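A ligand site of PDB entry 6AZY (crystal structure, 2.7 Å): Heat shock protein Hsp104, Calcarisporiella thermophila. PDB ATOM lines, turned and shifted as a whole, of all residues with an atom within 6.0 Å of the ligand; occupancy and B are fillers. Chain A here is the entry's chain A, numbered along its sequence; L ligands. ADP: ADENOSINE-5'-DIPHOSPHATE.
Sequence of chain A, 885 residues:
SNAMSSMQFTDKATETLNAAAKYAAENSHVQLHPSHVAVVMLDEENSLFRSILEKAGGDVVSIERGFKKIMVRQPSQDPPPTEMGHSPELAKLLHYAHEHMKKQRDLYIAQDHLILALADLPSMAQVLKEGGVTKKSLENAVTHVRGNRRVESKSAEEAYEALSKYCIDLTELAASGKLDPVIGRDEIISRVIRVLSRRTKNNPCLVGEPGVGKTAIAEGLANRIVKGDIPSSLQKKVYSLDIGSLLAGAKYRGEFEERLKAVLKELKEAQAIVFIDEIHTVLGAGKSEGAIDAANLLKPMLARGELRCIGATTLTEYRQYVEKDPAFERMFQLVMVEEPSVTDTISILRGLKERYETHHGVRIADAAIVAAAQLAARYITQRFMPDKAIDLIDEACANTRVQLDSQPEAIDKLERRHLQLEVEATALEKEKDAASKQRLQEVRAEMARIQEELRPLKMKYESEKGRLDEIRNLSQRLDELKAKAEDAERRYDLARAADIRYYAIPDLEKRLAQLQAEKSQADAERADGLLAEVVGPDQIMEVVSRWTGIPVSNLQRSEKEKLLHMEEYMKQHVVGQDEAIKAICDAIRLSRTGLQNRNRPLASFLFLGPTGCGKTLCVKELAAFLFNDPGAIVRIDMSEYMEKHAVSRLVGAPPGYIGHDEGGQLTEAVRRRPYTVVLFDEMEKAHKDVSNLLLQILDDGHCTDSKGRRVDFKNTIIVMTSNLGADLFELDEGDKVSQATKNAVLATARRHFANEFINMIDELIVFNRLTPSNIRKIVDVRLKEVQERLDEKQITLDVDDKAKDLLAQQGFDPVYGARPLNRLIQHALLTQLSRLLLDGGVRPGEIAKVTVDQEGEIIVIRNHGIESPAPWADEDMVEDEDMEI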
ATOM      1  N   ASP A 180     -35.324  16.362  -1.482  1.00  0.00           N
ATOM      2  CA  ASP A 180     -36.234  17.309  -0.837  1.00  0.00           C
ATOM      3  C   ASP A 180     -36.136  18.679  -1.488  1.00  0.00           C
ATOM      4  O   ASP A 180     -35.145  19.015  -2.131  1.00  0.00           O
ATOM      5  CB  ASP A 180     -35.928  17.469   0.657  1.00  0.00           C
ATOM      6  CG  ASP A 180     -36.368  16.286   1.507  1.00  0.00           C
ATOM      7  OD1 ASP A 180     -37.317  15.569   1.133  1.00  0.00           O
ATOM      8  OD2 ASP A 180     -35.793  16.124   2.606  1.00  0.00           O
ATOM      9  N   PRO A 181     -37.153  19.515  -1.291  1.00  0.00           N
ATOM     10  CA  PRO A 181     -37.087  20.881  -1.815  1.00  0.00           C
ATOM     11  C   PRO A 181     -36.010  21.693  -1.121  1.00  0.00           C
ATOM     12  O   PRO A 181     -35.738  21.495   0.061  1.00  0.00           O
ATOM     13  CB  PRO A 181     -38.489  21.440  -1.500  1.00  0.00           C
ATOM     14  CG  PRO A 181     -39.347  20.231  -1.348  1.00  0.00           C
ATOM     15  CD  PRO A 181     -38.491  19.185  -0.748  1.00  0.00           C
ATOM     16  N   VAL A 182     -35.448  22.664  -1.834  1.00  0.00           N
ATOM     17  CA  VAL A 182     -34.509  23.630  -1.264  1.00  0.00           C
ATOM     18  C   VAL A 182     -35.211  24.986  -1.231  1.00  0.00           C
ATOM     19  O   VAL A 182     -35.593  25.529  -2.273  1.00  0.00           O
ATOM     20  CB  VAL A 182     -33.203  23.691  -2.066  1.00  0.00           C
ATOM     21  CG1 VAL A 182     -32.265  24.675  -1.435  1.00  0.00           C
ATOM     22  CG2 VAL A 182     -32.562  22.291  -2.203  1.00  0.00           C
ATOM     23  N   ILE A 183     -35.373  25.553  -0.033  1.00  0.00           N
ATOM     24  CA  ILE A 183     -36.211  26.730   0.196  1.00  0.00           C
ATOM     25  C   ILE A 183     -35.317  27.899   0.589  1.00  0.00           C
ATOM     26  O   ILE A 183     -34.378  27.753   1.369  1.00  0.00           O
ATOM     27  CB  ILE A 183     -37.299  26.444   1.279  1.00  0.00           C
ATOM     28  CG1 ILE A 183     -38.381  25.516   0.760  1.00  0.00           C
ATOM     29  CG2 ILE A 183     -37.948  27.694   1.828  1.00  0.00           C
ATOM     30  CD1 ILE A 183     -38.071  24.067   0.983  1.00  0.00           C
ATOM     31  N   GLY A 184     -35.608  29.066   0.011  1.00  0.00           N
ATOM     32  CA  GLY A 184     -34.980  30.287   0.501  1.00  0.00           C
ATOM     33  C   GLY A 184     -33.510  30.497   0.188  1.00  0.00           C
ATOM     34  O   GLY A 184     -32.872  31.297   0.886  1.00  0.00           O
ATOM     35  N   ARG A 185     -32.969  29.839  -0.854  1.00  0.00           N
ATOM     36  CA  ARG A 185     -31.593  30.033  -1.299  1.00  0.00           C
ATOM     37  C   ARG A 185     -31.501  30.461  -2.766  1.00  0.00           C
ATOM     38  O   ARG A 185     -30.494  30.192  -3.416  1.00  0.00           O
ATOM     39  CB  ARG A 185     -30.730  28.774  -1.110  1.00  0.00           C
ATOM     40  CG  ARG A 185     -30.448  28.284   0.266  1.00  0.00           C
ATOM     41  CD  ARG A 185     -29.660  29.325   1.061  1.00  0.00           C
ATOM     42  NE  ARG A 185     -29.074  28.797   2.292  1.00  0.00           N
ATOM     43  CZ  ARG A 185     -28.453  29.525   3.220  1.00  0.00           C
ATOM     44  NH1 ARG A 185     -28.397  30.862   3.106  1.00  0.00           N
ATOM     45  NH2 ARG A 185     -27.921  28.938   4.278  1.00  0.00           N
ATOM     46  N   GLY A 208     -19.160  27.707   4.429  1.00  0.00           N
ATOM     47  CA  GLY A 208     -19.987  27.897   5.604  1.00  0.00           C
ATOM     48  C   GLY A 208     -19.758  26.746   6.563  1.00  0.00           C
ATOM     49  O   GLY A 208     -18.989  25.811   6.287  1.00  0.00           O
ATOM     50  N   GLU A 209     -20.425  26.829   7.690  1.00  0.00           N
ATOM     51  CA  GLU A 209     -20.245  25.874   8.776  1.00  0.00           C
ATOM     52  C   GLU A 209     -21.127  24.648   8.589  1.00  0.00           C
ATOM     53  O   GLU A 209     -22.001  24.633   7.722  1.00  0.00           O
ATOM     54  CB  GLU A 209     -20.431  26.616  10.092  1.00  0.00           C
ATOM     55  CG  GLU A 209     -19.122  27.363  10.397  1.00  0.00           C
ATOM     56  CD  GLU A 209     -19.176  28.238  11.605  1.00  0.00           C
ATOM     57  OE1 GLU A 209     -20.302  28.528  12.046  1.00  0.00           O
ATOM     58  OE2 GLU A 209     -18.112  28.613  12.138  1.00  0.00           O
ATOM     59  N   PRO A 210     -20.858  23.571   9.328  1.00  0.00           N
ATOM     60  CA  PRO A 210     -21.576  22.306   9.085  1.00  0.00           C
ATOM     61  C   PRO A 210     -23.062  22.451   9.347  1.00  0.00           C
ATOM     62  O   PRO A 210     -23.489  22.876  10.424  1.00  0.00           O
ATOM     63  CB  PRO A 210     -20.942  21.339  10.087  1.00  0.00           C
ATOM     64  CG  PRO A 210     -19.630  21.921  10.415  1.00  0.00           C
ATOM     65  CD  PRO A 210     -19.833  23.408  10.371  1.00  0.00           C
ATOM     66  N   GLY A 211     -23.860  22.058   8.353  1.00  0.00           N
ATOM     67  CA  GLY A 211     -25.306  22.041   8.487  1.00  0.00           C
ATOM     68  C   GLY A 211     -26.032  23.258   7.948  1.00  0.00           C
ATOM     69  O   GLY A 211     -27.265  23.251   7.969  1.00  0.00           O
ATOM     70  N   VAL A 212     -25.314  24.292   7.489  1.00  0.00           N
ATOM     71  CA  VAL A 212     -25.969  25.496   6.976  1.00  0.00           C
ATOM     72  C   VAL A 212     -26.634  25.303   5.610  1.00  0.00           C
ATOM     73  O   VAL A 212     -27.380  26.192   5.178  1.00  0.00           O
ATOM     74  CB  VAL A 212     -24.960  26.660   6.841  1.00  0.00           C
ATOM     75  CG1 VAL A 212     -24.271  26.959   8.182  1.00  0.00           C
ATOM     76  CG2 VAL A 212     -23.969  26.353   5.768  1.00  0.00           C
ATOM     77  N   GLY A 213     -26.369  24.186   4.937  1.00  0.00           N
ATOM     78  CA  GLY A 213     -26.913  23.890   3.632  1.00  0.00           C
ATOM     79  C   GLY A 213     -25.986  24.093   2.448  1.00  0.00           C
ATOM     80  O   GLY A 213     -26.453  24.519   1.378  1.00  0.00           O
ATOM     81  N   LYS A 214     -24.698  23.826   2.582  1.00  0.00           N
ATOM     82  CA  LYS A 214     -23.838  23.973   1.403  1.00  0.00           C
ATOM     83  C   LYS A 214     -24.174  22.906   0.373  1.00  0.00           C
ATOM     84  O   LYS A 214     -24.306  23.213  -0.814  1.00  0.00           O
ATOM     85  CB  LYS A 214     -22.387  23.897   1.798  1.00  0.00           C
ATOM     86  CG  LYS A 214     -21.973  25.035   2.677  1.00  0.00           C
ATOM     87  CD  LYS A 214     -20.533  24.869   2.980  1.00  0.00           C
ATOM     88  CE  LYS A 214     -20.260  23.690   3.906  1.00  0.00           C
ATOM     89  NZ  LYS A 214     -20.732  23.942   5.278  1.00  0.00           N
ATOM     90  N   THR A 215     -24.360  21.664   0.813  1.00  0.00           N
ATOM     91  CA  THR A 215     -24.769  20.611  -0.114  1.00  0.00           C
ATOM     92  C   THR A 215     -26.139  20.881  -0.716  1.00  0.00           C
ATOM     93  O   THR A 215     -26.385  20.522  -1.870  1.00  0.00           O
ATOM     94  CB  THR A 215     -24.725  19.260   0.588  1.00  0.00           C
ATOM     95  OG1 THR A 215     -23.389  19.035   1.047  1.00  0.00           O
ATOM     96  CG2 THR A 215     -25.095  18.142  -0.359  1.00  0.00           C
ATOM     97  N   ALA A 216     -27.056  21.492   0.049  1.00  0.00           N
ATOM     98  CA  ALA A 216     -28.385  21.737  -0.486  1.00  0.00           C
ATOM     99  C   ALA A 216     -28.344  22.745  -1.635  1.00  0.00           C
ATOM    100  O   ALA A 216     -29.147  22.660  -2.576  1.00  0.00           O
ATOM    101  CB  ALA A 216     -29.324  22.218   0.623  1.00  0.00           C
ATOM    102  N   ILE A 217     -27.407  23.681  -1.592  1.00  0.00           N
ATOM    103  CA  ILE A 217     -27.225  24.622  -2.696  1.00  0.00           C
ATOM    104  C   ILE A 217     -26.728  23.921  -3.956  1.00  0.00           C
ATOM    105  O   ILE A 217     -27.194  24.227  -5.053  1.00  0.00           O
ATOM    106  CB  ILE A 217     -26.292  25.749  -2.243  1.00  0.00           C
ATOM    107  CG1 ILE A 217     -27.051  26.615  -1.237  1.00  0.00           C
ATOM    108  CG2 ILE A 217     -25.759  26.483  -3.423  1.00  0.00           C
ATOM    109  CD1 ILE A 217     -26.220  27.568  -0.461  1.00  0.00           C
ATOM    110  N   GLU A 219     -27.478  20.739  -4.519  1.00  0.00           N
ATOM    111  CA  GLU A 219     -28.689  19.992  -4.867  1.00  0.00           C
ATOM    112  C   GLU A 219     -29.736  20.889  -5.527  1.00  0.00           C
ATOM    113  O   GLU A 219     -30.393  20.475  -6.479  1.00  0.00           O
ATOM    114  CB  GLU A 219     -29.297  19.310  -3.621  1.00  0.00           C
ATOM    115  CG  GLU A 219     -28.441  18.132  -3.022  1.00  0.00           C
ATOM    116  CD  GLU A 219     -29.036  17.477  -1.742  1.00  0.00           C
ATOM    117  OE1 GLU A 219     -30.045  17.974  -1.188  1.00  0.00           O
ATOM    118  OE2 GLU A 219     -28.480  16.435  -1.310  1.00  0.00           O
ATOM    119  N   PHE A 275     -19.333  18.740  -7.935  1.00  0.00           N
ATOM    120  CA  PHE A 275     -19.402  19.221  -6.570  1.00  0.00           C
ATOM    121  C   PHE A 275     -18.473  18.383  -5.713  1.00  0.00           C
ATOM    122  O   PHE A 275     -18.499  17.145  -5.794  1.00  0.00           O
ATOM    123  CB  PHE A 275     -20.852  19.139  -6.073  1.00  0.00           C
ATOM    124  CG  PHE A 275     -21.019  19.531  -4.641  1.00  0.00           C
ATOM    125  CD1 PHE A 275     -20.880  20.857  -4.244  1.00  0.00           C
ATOM    126  CD2 PHE A 275     -21.389  18.579  -3.693  1.00  0.00           C
ATOM    127  CE1 PHE A 275     -21.049  21.220  -2.924  1.00  0.00           C
ATOM    128  CE2 PHE A 275     -21.568  18.928  -2.387  1.00  0.00           C
ATOM    129  CZ  PHE A 275     -21.399  20.264  -2.000  1.00  0.00           C
ATOM    130  N   ASP A 277     -17.573  18.139  -1.801  1.00  0.00           N
ATOM    131  CA  ASP A 277     -17.668  18.448  -0.387  1.00  0.00           C
ATOM    132  C   ASP A 277     -16.328  18.156   0.282  1.00  0.00           C
ATOM    133  O   ASP A 277     -15.613  17.222  -0.079  1.00  0.00           O
ATOM    134  CB  ASP A 277     -18.764  17.606   0.249  1.00  0.00           C
ATOM    135  CG  ASP A 277     -19.194  18.120   1.608  1.00  0.00           C
ATOM    136  OD1 ASP A 277     -18.768  19.217   2.034  1.00  0.00           O
ATOM    137  OD2 ASP A 277     -19.942  17.376   2.280  1.00  0.00           O
ATOM    138  N   ALA A 312     -17.016  22.863  -1.420  1.00  0.00           N
ATOM    139  CA  ALA A 312     -17.614  23.202  -0.146  1.00  0.00           C
ATOM    140  C   ALA A 312     -16.591  22.971   0.953  1.00  0.00           C
ATOM    141  O   ALA A 312     -15.831  22.015   0.913  1.00  0.00           O
ATOM    142  CB  ALA A 312     -18.874  22.402   0.119  1.00  0.00           C
ATOM    143  N   ILE A 348     -37.824  27.177   5.933  1.00  0.00           N
ATOM    144  CA  ILE A 348     -37.273  25.922   5.440  1.00  0.00           C
ATOM    145  C   ILE A 348     -38.097  24.749   5.960  1.00  0.00           C
ATOM    146  O   ILE A 348     -38.406  23.823   5.211  1.00  0.00           O
ATOM    147  CB  ILE A 348     -35.786  25.809   5.804  1.00  0.00           C
ATOM    148  CG1 ILE A 348     -35.023  26.888   5.036  1.00  0.00           C
ATOM    149  CG2 ILE A 348     -35.281  24.407   5.494  1.00  0.00           C
ATOM    150  CD1 ILE A 348     -33.604  27.086   5.475  1.00  0.00           C
ATOM    151  N   LEU A 352     -40.156  21.719   3.904  1.00  0.00           N
ATOM    152  CA  LEU A 352     -39.872  20.296   4.076  1.00  0.00           C
ATOM    153  C   LEU A 352     -41.014  19.517   4.737  1.00  0.00           C
ATOM    154  O   LEU A 352     -41.031  18.285   4.666  1.00  0.00           O
ATOM    155  CB  LEU A 352     -38.603  20.145   4.909  1.00  0.00           C
ATOM    156  CG  LEU A 352     -37.325  20.771   4.343  1.00  0.00           C
ATOM    157  CD1 LEU A 352     -36.223  20.688   5.398  1.00  0.00           C
ATOM    158  CD2 LEU A 352     -36.908  20.060   3.115  1.00  0.00           C
ATOM    159  N   TYR A 356     -41.675  15.093   5.405  1.00  0.00           N
ATOM    160  CA  TYR A 356     -41.609  14.250   6.588  1.00  0.00           C
ATOM    161  C   TYR A 356     -42.974  13.703   6.978  1.00  0.00           C
ATOM    162  O   TYR A 356     -43.067  12.548   7.405  1.00  0.00           O
ATOM    163  CB  TYR A 356     -40.961  14.941   7.801  1.00  0.00           C
ATOM    164  CG  TYR A 356     -39.503  15.314   7.601  1.00  0.00           C
ATOM    165  CD1 TYR A 356     -38.958  15.478   6.360  1.00  0.00           C
ATOM    166  CD2 TYR A 356     -38.616  15.102   8.635  1.00  0.00           C
ATOM    167  CE1 TYR A 356     -37.629  15.716   6.169  1.00  0.00           C
ATOM    168  CE2 TYR A 356     -37.259  15.285   8.460  1.00  0.00           C
ATOM    169  CZ  TYR A 356     -36.778  15.589   7.199  1.00  0.00           C
ATOM    170  OH  TYR A 356     -35.435  15.787   6.969  1.00  0.00           O
ATOM    171  N   PRO A 386     -29.998  24.851   9.171  1.00  0.00           N
ATOM    172  CA  PRO A 386     -31.255  24.244   9.631  1.00  0.00           C
ATOM    173  C   PRO A 386     -31.134  22.773  10.063  1.00  0.00           C
ATOM    174  O   PRO A 386     -32.127  22.210  10.488  1.00  0.00           O
ATOM    175  CB  PRO A 386     -32.155  24.341   8.380  1.00  0.00           C
ATOM    176  CG  PRO A 386     -31.198  24.277   7.240  1.00  0.00           C
ATOM    177  CD  PRO A 386     -29.934  24.975   7.707  1.00  0.00           C
ATOM    178  N   ASP A 387     -29.938  22.183   9.936  1.00  0.00           N
ATOM    179  CA  ASP A 387     -29.737  20.759  10.197  1.00  0.00           C
ATOM    180  C   ASP A 387     -30.300  20.371  11.560  1.00  0.00           C
ATOM    181  O   ASP A 387     -31.080  19.427  11.678  1.00  0.00           O
ATOM    182  CB  ASP A 387     -28.234  20.422  10.070  1.00  0.00           C
ATOM    183  CG  ASP A 387     -27.928  18.934  10.178  1.00  0.00           C
ATOM    184  OD1 ASP A 387     -28.285  18.152   9.265  1.00  0.00           O
ATOM    185  OD2 ASP A 387     -27.243  18.553  11.151  1.00  0.00           O
ATOM    186  N   ILE A 390     -34.465  20.453  11.601  1.00  0.00           N
ATOM    187  CA  ILE A 390     -34.848  19.305  10.811  1.00  0.00           C
ATOM    188  C   ILE A 390     -34.645  18.061  11.661  1.00  0.00           C
ATOM    189  O   ILE A 390     -35.492  17.169  11.708  1.00  0.00           O
ATOM    190  CB  ILE A 390     -33.984  19.235   9.542  1.00  0.00           C
ATOM    191  CG1 ILE A 390     -34.237  20.475   8.696  1.00  0.00           C
ATOM    192  CG2 ILE A 390     -34.218  17.941   8.772  1.00  0.00           C
ATOM    193  CD1 ILE A 390     -33.266  20.673   7.558  1.00  0.00           C
HETATM  194  PB  ADP L   1     -23.804  21.202   4.708  1.00  0.00           P
HETATM  195  O1B ADP L   1     -23.418  22.584   4.791  1.00  0.00           O
HETATM  196  O2B ADP L   1     -23.119  20.449   5.755  1.00  0.00           O
HETATM  197  O3B ADP L   1     -23.511  20.638   3.369  1.00  0.00           O
HETATM  198  PA  ADP L   1     -26.526  20.291   4.170  1.00  0.00           P
HETATM  199  O1A ADP L   1     -26.684  20.764   2.730  1.00  0.00           O
HETATM  200  O2A ADP L   1     -26.275  18.828   4.241  1.00  0.00           O
HETATM  201  O3A ADP L   1     -25.381  21.109   4.922  1.00  0.00           O
HETATM  202  O5' ADP L   1     -27.782  20.703   5.003  1.00  0.00           O
HETATM  203  C5' ADP L   1     -28.130  20.076   6.241  1.00  0.00           C
HETATM  204  C4' ADP L   1     -29.529  19.522   6.167  1.00  0.00           C
HETATM  205  O4' ADP L   1     -30.467  20.617   6.007  1.00  0.00           O
HETATM  206  C3' ADP L   1     -29.808  18.569   5.001  1.00  0.00           C
HETATM  207  O3' ADP L   1     -30.863  17.659   5.311  1.00  0.00           O
HETATM  208  C2' ADP L   1     -30.321  19.507   3.914  1.00  0.00           C
HETATM  209  O2' ADP L   1     -31.193  18.813   3.038  1.00  0.00           O
HETATM  210  C1' ADP L   1     -31.104  20.530   4.740  1.00  0.00           C
HETATM  211  N9  ADP L   1     -31.129  21.875   4.175  1.00  0.00           N
HETATM  212  C8  ADP L   1     -30.159  22.832   4.259  1.00  0.00           C
HETATM  213  N7  ADP L   1     -30.512  23.994   3.745  1.00  0.00           N
HETATM  214  C5  ADP L   1     -31.793  23.770   3.284  1.00  0.00           C
HETATM  215  C6  ADP L   1     -32.718  24.588   2.602  1.00  0.00           C
HETATM  216  N6  ADP L   1     -32.462  25.845   2.253  1.00  0.00           N
HETATM  217  N1  ADP L   1     -33.909  24.047   2.279  1.00  0.00           N
HETATM  218  C2  ADP L   1     -34.142  22.769   2.589  1.00  0.00           C
HETATM  219  N3  ADP L   1     -33.349  21.902   3.208  1.00  0.00           N
HETATM  220  C4  ADP L   1     -32.189  22.469   3.533  1.00  0.00           C
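O1A of the ligand is in hydrogen-bond range of N of Ala 216 (2.8 Å). N of Thr 215 sits at hydrogen-bond distance from O3B of the ligand. The side-chain hydroxyl of Thr 215 lies within hydrogen-bond range of an oxygen (O3B) of the ligand, 2.8 Å away. An oxygen (O1B) of the ligand lies within hydrogen-bond range of the backbone NH (N) of Lys 214 (2.8 Å). The side-chain amino group (NZ) of Lys 214 is in salt-bridge range of an oxygen (O1B) of the ligand, 3.0 Å away. N1 of the ligand sits at hydrogen-bond distance from N of Ile 183 (3.1 Å). The backbone carbonyl oxygen (O) of Ile 183 is in hydrogen-bond range of a nitrogen (N6) of the ligand (2.8 Å). The backbone NH (N) of Gly 211 sits at hydrogen-bond distance from an oxygen (O2B) of the ligand, 3.1 Å away. O3A of the ligand is in hydrogen-bond range of N of Gly 213, 3.2 Å away.
The side-chain amino group of Lys 214 lies within hydrogen-bond range of the backbone carbonyl oxygen of Glu 209, at 2.8 Å. The backbone carbonyl oxygen of Gly 208 is in hydrogen-bond range of the side-chain amino group of Lys 214 (2.7 Å). The backbone carbonyl oxygen (O) of Gly 211 lies within hydrogen-bond range of the backbone NH (N) of Asp 387 (3.5 Å). The guanidinium group (NH2) of Arg 185 is in hydrogen-bond range of the backbone carbonyl oxygen (O) of Val 212, 2.9 Å away.
O of Pro 181 touches C2 of the ligand, at 3.2 Å. CA of Val 182 touches N1 of the ligand, 3.6 Å away. Arg 185 touches the ligand. Glu 209 touches the ligand (O to O1B, 3.8 Å). Val 212 touches the ligand (N to O1B, 3.7 Å). CG2 of Ile 348 touches N1 of the ligand (3.5 Å). Leu 352 touches the ligand (CD1 to N3, 3.8 Å). CG of Pro 386 touches C8 of the ligand (3.5 Å). Asp 387 touches the ligand (OD1 to C5', 3.6 Å). Ile 390 touches the ligand. Hydrophobic or aromatic side chains within 4 Å of the ligand: Val 182, Val 212, Ala 216, Ile 348, Leu 352, Pro 386 and Ile 390. The nearest printed residue that does not touch the ligand is Pro 210 (4.1 Å).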
